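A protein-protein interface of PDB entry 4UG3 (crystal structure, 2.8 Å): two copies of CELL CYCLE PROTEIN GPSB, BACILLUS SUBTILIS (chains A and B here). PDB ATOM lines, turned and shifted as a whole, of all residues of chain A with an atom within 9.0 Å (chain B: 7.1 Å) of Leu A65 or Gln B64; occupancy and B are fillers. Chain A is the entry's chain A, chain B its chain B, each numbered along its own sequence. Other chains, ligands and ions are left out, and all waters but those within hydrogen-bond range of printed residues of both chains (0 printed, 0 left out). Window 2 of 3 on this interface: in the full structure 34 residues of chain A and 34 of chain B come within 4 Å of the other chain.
The side-chain amide nitrogen (ND2) of Asn A58 is in hydrogen-bond range of the side-chain carboxylate (OE1) of Glu B57 (2.7 Å). NZ of Lys A62 lies within salt-bridge range of OE2 of Glu B57.
O of Gln B60 sits at hydrogen-bond distance from NE2 of Gln B64, at 2.9 Å.
Among the printed residues, merely in contact across the chains: Asn A58 with Leu B61 (3.4 Å), Leu A61 with Leu B61 (3.9 Å), Leu A61 with Leu B65 (3.9 Å), Lys A62 with Leu B61 (3.9 Å), Leu A65 with Leu B61 (3.8 Å) and Leu A65 with Gln B64 (3.9 Å).
Of the printed residues of chain B, Leu A65 touches Leu B61 and Gln B64. Of chain A, only Leu A65 comes within 4 Å of Gln B64. Of the printed residues of chain A, Leu B61 touches Asn A58, Leu A61, Lys A62 and Leu A65. Of the printed residues of chain B, Leu A61 touches Leu B61 (3.9 Å) and Leu B65 (3.9 Å). Printed residues of chain B within 4 Å of Asn A58: Glu B57 (2.7 Å) and Leu B61 (3.4 Å). Of the printed residues of chain A, Glu B57 touches Asn A58 (2.7 Å) and Lys A62 (2.4 Å). Leu A59 touches none of the printed residues of chain B. Glu B66 touches none of the printed residues of chain A. The nearest residue of chain A that does not touch Gln B64 is Lys A62 (7.2 Å). The nearest printed residue of chain A that does not touch Leu B61 is Leu A59 (5.4 Å).
Of the 10 printed residues of chain B, 4 touch a printed residue of chain A. Printed residues of chain B that touch a printed residue of chain A: Glu B57, Leu B61, Gln B64 and Leu B65. Hydrophobic or aromatic side chains of chain B within 4 Å of the printed part of chain A: Leu B61 and Leu B65. Among the printed residues, 8 pairs touch across the chains.
Leu A61 touches its own counterpart, Leu B61. Leu A61 touches Leu B65, and with the chains exchanged Leu A65 touches Leu B61. Lys A62 touches Leu B61, but with the chains exchanged Leu A61 does not touch Lys B62 (4.4 Å). Leu A65 touches Gln B64, but with the chains exchanged Gln A64 does not touch Leu B65 (4.03 Å). Positions printed for both chains: 59, 60, 61, 62, 63, 64, 65, 66 and 67.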
ATOM      1  N   ASN A  58      11.712  -1.521   9.947  1.00  0.00           N
ATOM      2  CA  ASN A  58      10.447  -1.516   9.190  1.00  0.00           C
ATOM      3  C   ASN A  58       9.358  -0.660   9.852  1.00  0.00           C
ATOM      4  O   ASN A  58       8.529  -0.061   9.168  1.00  0.00           O
ATOM      5  CB  ASN A  58       9.968  -2.945   8.885  1.00  0.00           C
ATOM      6  CG  ASN A  58      10.892  -3.695   7.873  1.00  0.00           C
ATOM      7  OD1 ASN A  58      11.852  -3.129   7.317  1.00  0.00           O
ATOM      8  ND2 ASN A  58      10.600  -4.983   7.645  1.00  0.00           N
ATOM      9  N   LEU A  59       9.397  -0.565  11.178  1.00  0.00           N
ATOM     10  CA  LEU A  59       8.531   0.356  11.922  1.00  0.00           C
ATOM     11  C   LEU A  59       8.900   1.814  11.696  1.00  0.00           C
ATOM     12  O   LEU A  59       8.007   2.640  11.532  1.00  0.00           O
ATOM     13  CB  LEU A  59       8.554   0.050  13.420  1.00  0.00           C
ATOM     14  CG  LEU A  59       7.520  -0.949  13.964  1.00  0.00           C
ATOM     15  CD1 LEU A  59       7.425  -2.274  13.201  1.00  0.00           C
ATOM     16  CD2 LEU A  59       7.880  -1.207  15.411  1.00  0.00           C
ATOM     17  N   GLN A  60      10.200   2.127  11.724  1.00  0.00           N
ATOM     18  CA  GLN A  60      10.701   3.454  11.321  1.00  0.00           C
ATOM     19  C   GLN A  60      10.137   3.862   9.957  1.00  0.00           C
ATOM     20  O   GLN A  60       9.595   4.964   9.807  1.00  0.00           O
ATOM     21  CB  GLN A  60      12.232   3.482  11.228  1.00  0.00           C
ATOM     22  CG  GLN A  60      12.972   3.647  12.546  1.00  0.00           C
ATOM     23  CD  GLN A  60      14.496   3.699  12.358  1.00  0.00           C
ATOM     24  OE1 GLN A  60      15.172   2.656  12.222  1.00  0.00           O
ATOM     25  NE2 GLN A  60      15.045   4.924  12.358  1.00  0.00           N
ATOM     26  N   LEU A  61      10.266   2.965   8.978  1.00  0.00           N
ATOM     27  CA  LEU A  61       9.912   3.274   7.578  1.00  0.00           C
ATOM     28  C   LEU A  61       8.428   3.609   7.408  1.00  0.00           C
ATOM     29  O   LEU A  61       8.066   4.445   6.561  1.00  0.00           O
ATOM     30  CB  LEU A  61      10.333   2.138   6.607  1.00  0.00           C
ATOM     31  CG  LEU A  61      11.848   1.940   6.363  1.00  0.00           C
ATOM     32  CD1 LEU A  61      12.160   0.556   5.829  1.00  0.00           C
ATOM     33  CD2 LEU A  61      12.419   2.985   5.425  1.00  0.00           C
ATOM     34  N   LYS A  62       7.589   2.971   8.226  1.00  0.00           N
ATOM     35  CA  LYS A  62       6.141   3.179   8.185  1.00  0.00           C
ATOM     36  C   LYS A  62       5.703   4.486   8.826  1.00  0.00           C
ATOM     37  O   LYS A  62       4.711   5.062   8.392  1.00  0.00           O
ATOM     38  CB  LYS A  62       5.412   2.005   8.847  1.00  0.00           C
ATOM     39  CG  LYS A  62       5.280   0.791   7.949  1.00  0.00           C
ATOM     40  CD  LYS A  62       5.147  -0.483   8.762  1.00  0.00           C
ATOM     41  CE  LYS A  62       4.585  -1.617   7.918  1.00  0.00           C
ATOM     42  NZ  LYS A  62       4.996  -2.956   8.396  1.00  0.00           N
ATOM     43  N   LYS A  63       6.398   4.913   9.884  1.00  0.00           N
ATOM     44  CA  LYS A  63       6.203   6.253  10.471  1.00  0.00           C
ATOM     45  C   LYS A  63       6.342   7.314   9.376  1.00  0.00           C
ATOM     46  O   LYS A  63       5.441   8.120   9.160  1.00  0.00           O
ATOM     47  CB  LYS A  63       7.222   6.532  11.587  1.00  0.00           C
ATOM     48  CG  LYS A  63       6.717   6.376  13.023  1.00  0.00           C
ATOM     49  CD  LYS A  63       7.892   6.193  13.997  1.00  0.00           C
ATOM     50  CE  LYS A  63       7.914   7.162  15.172  1.00  0.00           C
ATOM     51  NZ  LYS A  63       7.312   6.584  16.397  1.00  0.00           N
ATOM     52  N   GLN A  64       7.466   7.269   8.672  1.00  0.00           N
ATOM     53  CA  GLN A  64       7.741   8.150   7.533  1.00  0.00           C
ATOM     54  C   GLN A  64       6.673   8.108   6.412  1.00  0.00           C
ATOM     55  O   GLN A  64       6.438   9.120   5.751  1.00  0.00           O
ATOM     56  CB  GLN A  64       9.141   7.854   6.969  1.00  0.00           C
ATOM     57  CG  GLN A  64      10.243   8.273   7.936  1.00  0.00           C
ATOM     58  CD  GLN A  64      11.615   7.756   7.567  1.00  0.00           C
ATOM     59  OE1 GLN A  64      12.263   8.277   6.663  1.00  0.00           O
ATOM     60  NE2 GLN A  64      12.081   6.747   8.295  1.00  0.00           N
ATOM     61  N   LEU A  65       6.024   6.960   6.217  1.00  0.00           N
ATOM     62  CA  LEU A  65       4.906   6.824   5.250  1.00  0.00           C
ATOM     63  C   LEU A  65       3.548   7.477   5.613  1.00  0.00           C
ATOM     64  O   LEU A  65       2.654   7.508   4.771  1.00  0.00           O
ATOM     65  CB  LEU A  65       4.663   5.346   4.909  1.00  0.00           C
ATOM     66  CG  LEU A  65       5.512   4.814   3.768  1.00  0.00           C
ATOM     67  CD1 LEU A  65       5.568   3.303   3.855  1.00  0.00           C
ATOM     68  CD2 LEU A  65       4.974   5.254   2.408  1.00  0.00           C
ATOM     69  N   GLU A  66       3.374   8.004   6.822  1.00  0.00           N
ATOM     70  CA  GLU A  66       2.095   8.636   7.162  1.00  0.00           C
ATOM     71  C   GLU A  66       1.880   9.981   6.443  1.00  0.00           C
ATOM     72  O   GLU A  66       0.762  10.492   6.399  1.00  0.00           O
ATOM     73  CB  GLU A  66       1.979   8.830   8.669  1.00  0.00           C
ATOM     74  CG  GLU A  66       1.988   7.534   9.474  1.00  0.00           C
ATOM     75  CD  GLU A  66       2.405   7.741  10.926  1.00  0.00           C
ATOM     76  OE1 GLU A  66       2.996   8.804  11.250  1.00  0.00           O
ATOM     77  OE2 GLU A  66       2.150   6.831  11.751  1.00  0.00           O
ATOM     78  N   GLU A  67       2.953  10.534   5.878  1.00  0.00           N
ATOM     79  CA  GLU A  67       2.961  11.883   5.321  1.00  0.00           C
ATOM     80  C   GLU A  67       2.590  11.886   3.834  1.00  0.00           C
ATOM     81  O   GLU A  67       3.393  11.509   2.984  1.00  0.00           O
ATOM     82  CB  GLU A  67       4.342  12.524   5.566  1.00  0.00           C
ATOM     83  CG  GLU A  67       4.591  12.944   7.019  1.00  0.00           C
ATOM     84  CD  GLU A  67       4.922  11.797   7.974  1.00  0.00           C
ATOM     85  OE1 GLU A  67       4.452  10.663   7.767  1.00  0.00           O
ATOM     86  OE2 GLU A  67       5.650  12.030   8.966  1.00  0.00           O
ATOM     87  N   GLU B  57       9.920  -7.171   3.087  1.00  0.00           N
ATOM     88  CA  GLU B  57       9.092  -6.057   3.528  1.00  0.00           C
ATOM     89  C   GLU B  57       9.910  -4.748   3.612  1.00  0.00           C
ATOM     90  O   GLU B  57       9.414  -3.677   3.249  1.00  0.00           O
ATOM     91  CB  GLU B  57       8.487  -6.405   4.893  1.00  0.00           C
ATOM     92  CG  GLU B  57       7.364  -5.508   5.389  1.00  0.00           C
ATOM     93  CD  GLU B  57       7.285  -5.403   6.921  1.00  0.00           C
ATOM     94  OE1 GLU B  57       8.101  -6.009   7.656  1.00  0.00           O
ATOM     95  OE2 GLU B  57       6.393  -4.683   7.412  1.00  0.00           O
ATOM     96  N   LEU B  59      12.565  -3.825   1.751  1.00  0.00           N
ATOM     97  CA  LEU B  59      12.647  -3.379   0.358  1.00  0.00           C
ATOM     98  C   LEU B  59      11.311  -2.864  -0.241  1.00  0.00           C
ATOM     99  O   LEU B  59      11.304  -1.912  -1.024  1.00  0.00           O
ATOM    100  CB  LEU B  59      13.200  -4.497  -0.534  1.00  0.00           C
ATOM    101  CG  LEU B  59      14.729  -4.684  -0.622  1.00  0.00           C
ATOM    102  CD1 LEU B  59      15.492  -4.367   0.666  1.00  0.00           C
ATOM    103  CD2 LEU B  59      15.057  -6.098  -1.083  1.00  0.00           C
ATOM    104  N   GLN B  60      10.195  -3.489   0.113  1.00  0.00           N
ATOM    105  CA  GLN B  60       8.887  -2.997  -0.311  1.00  0.00           C
ATOM    106  C   GLN B  60       8.508  -1.662   0.327  1.00  0.00           C
ATOM    107  O   GLN B  60       7.673  -0.942  -0.211  1.00  0.00           O
ATOM    108  CB  GLN B  60       7.805  -4.017  -0.006  1.00  0.00           C
ATOM    109  CG  GLN B  60       7.933  -5.294  -0.832  1.00  0.00           C
ATOM    110  CD  GLN B  60       7.207  -6.505  -0.224  1.00  0.00           C
ATOM    111  OE1 GLN B  60       7.386  -7.631  -0.693  1.00  0.00           O
ATOM    112  NE2 GLN B  60       6.392  -6.280   0.820  1.00  0.00           N
ATOM    113  N   LEU B  61       9.089  -1.340   1.481  1.00  0.00           N
ATOM    114  CA  LEU B  61       8.837  -0.035   2.120  1.00  0.00           C
ATOM    115  C   LEU B  61       9.732   1.070   1.554  1.00  0.00           C
ATOM    116  O   LEU B  61       9.322   2.225   1.507  1.00  0.00           O
ATOM    117  CB  LEU B  61       8.961  -0.122   3.649  1.00  0.00           C
ATOM    118  CG  LEU B  61       7.880  -0.932   4.383  1.00  0.00           C
ATOM    119  CD1 LEU B  61       8.147  -0.967   5.890  1.00  0.00           C
ATOM    120  CD2 LEU B  61       6.484  -0.394   4.104  1.00  0.00           C
ATOM    121  N   LYS B  62      10.939   0.710   1.127  1.00  0.00           N
ATOM    122  CA  LYS B  62      11.836   1.657   0.460  1.00  0.00           C
ATOM    123  C   LYS B  62      11.347   2.062  -0.932  1.00  0.00           C
ATOM    124  O   LYS B  62      11.600   3.190  -1.380  1.00  0.00           O
ATOM    125  CB  LYS B  62      13.257   1.096   0.406  1.00  0.00           C
ATOM    126  CG  LYS B  62      13.936   1.166   1.763  1.00  0.00           C
ATOM    127  CD  LYS B  62      15.169   0.286   1.876  1.00  0.00           C
ATOM    128  CE  LYS B  62      15.868   0.569   3.207  1.00  0.00           C
ATOM    129  NZ  LYS B  62      16.777  -0.508   3.699  1.00  0.00           N
ATOM    130  N   LYS B  63      10.645   1.146  -1.599  1.00  0.00           N
ATOM    131  CA  LYS B  63      10.004   1.434  -2.877  1.00  0.00           C
ATOM    132  C   LYS B  63       8.882   2.432  -2.635  1.00  0.00           C
ATOM    133  O   LYS B  63       8.858   3.504  -3.233  1.00  0.00           O
ATOM    134  CB  LYS B  63       9.453   0.152  -3.530  1.00  0.00           C
ATOM    135  CG  LYS B  63       9.299   0.219  -5.049  1.00  0.00           C
ATOM    136  CD  LYS B  63      10.636  -0.005  -5.763  1.00  0.00           C
ATOM    137  CE  LYS B  63      10.566   0.221  -7.277  1.00  0.00           C
ATOM    138  NZ  LYS B  63      10.764   1.643  -7.694  1.00  0.00           N
ATOM    139  N   GLN B  64       7.977   2.093  -1.722  1.00  0.00           N
ATOM    140  CA  GLN B  64       6.831   2.950  -1.427  1.00  0.00           C
ATOM    141  C   GLN B  64       7.230   4.350  -0.975  1.00  0.00           C
ATOM    142  O   GLN B  64       6.480   5.294  -1.215  1.00  0.00           O
ATOM    143  CB  GLN B  64       5.904   2.292  -0.404  1.00  0.00           C
ATOM    144  CG  GLN B  64       5.145   1.113  -0.985  1.00  0.00           C
ATOM    145  CD  GLN B  64       4.333   0.363   0.054  1.00  0.00           C
ATOM    146  OE1 GLN B  64       3.123   0.568   0.167  1.00  0.00           O
ATOM    147  NE2 GLN B  64       4.991  -0.516   0.815  1.00  0.00           N
ATOM    148  N   LEU B  65       8.409   4.478  -0.353  1.00  0.00           N
ATOM    149  CA  LEU B  65       8.945   5.784   0.076  1.00  0.00           C
ATOM    150  C   LEU B  65       9.550   6.635  -1.047  1.00  0.00           C
ATOM    151  O   LEU B  65       9.514   7.868  -0.958  1.00  0.00           O
ATOM    152  CB  LEU B  65       9.956   5.648   1.228  1.00  0.00           C
ATOM    153  CG  LEU B  65       9.443   6.185   2.569  1.00  0.00           C
ATOM    154  CD1 LEU B  65      10.397   5.845   3.705  1.00  0.00           C
ATOM    155  CD2 LEU B  65       9.207   7.689   2.520  1.00  0.00           C
ATOM    156  N   GLU B  66      10.111   6.007  -2.081  1.00  0.00           N
ATOM    157  CA  GLU B  66      10.517   6.773  -3.263  1.00  0.00           C
ATOM    158  C   GLU B  66       9.319   7.115  -4.196  1.00  0.00           C
ATOM    159  O   GLU B  66       9.500   7.802  -5.207  1.00  0.00           O
ATOM    160  CB  GLU B  66      11.672   6.083  -4.002  1.00  0.00           C
ATOM    161  CG  GLU B  66      11.310   4.967  -4.972  1.00  0.00           C
ATOM    162  CD  GLU B  66      12.488   4.570  -5.840  1.00  0.00           C
ATOM    163  OE1 GLU B  66      12.935   5.414  -6.653  1.00  0.00           O
ATOM    164  OE2 GLU B  66      12.967   3.420  -5.702  1.00  0.00           O
ATOM    165  N   GLU B  67       8.118   6.644  -3.830  1.00  0.00           N
ATOM    166  CA  GLU B  67       6.883   6.849  -4.575  1.00  0.00           C
ATOM    167  C   GLU B  67       5.783   7.361  -3.630  1.00  0.00           C
ATOM    168  O   GLU B  67       5.948   8.375  -2.933  1.00  0.00           O
ATOM    169  CB  GLU B  67       6.465   5.519  -5.206  1.00  0.00           C
ATOM    170  CG  GLU B  67       7.574   4.861  -6.036  1.00  0.00           C
ATOM    171  CD  GLU B  67       7.251   3.461  -6.562  1.00  0.00           C
ATOM    172  OE1 GLU B  67       6.220   2.862  -6.171  1.00  0.00           O
ATOM    173  OE2 GLU B  67       8.052   2.938  -7.376  1.00  0.00           O
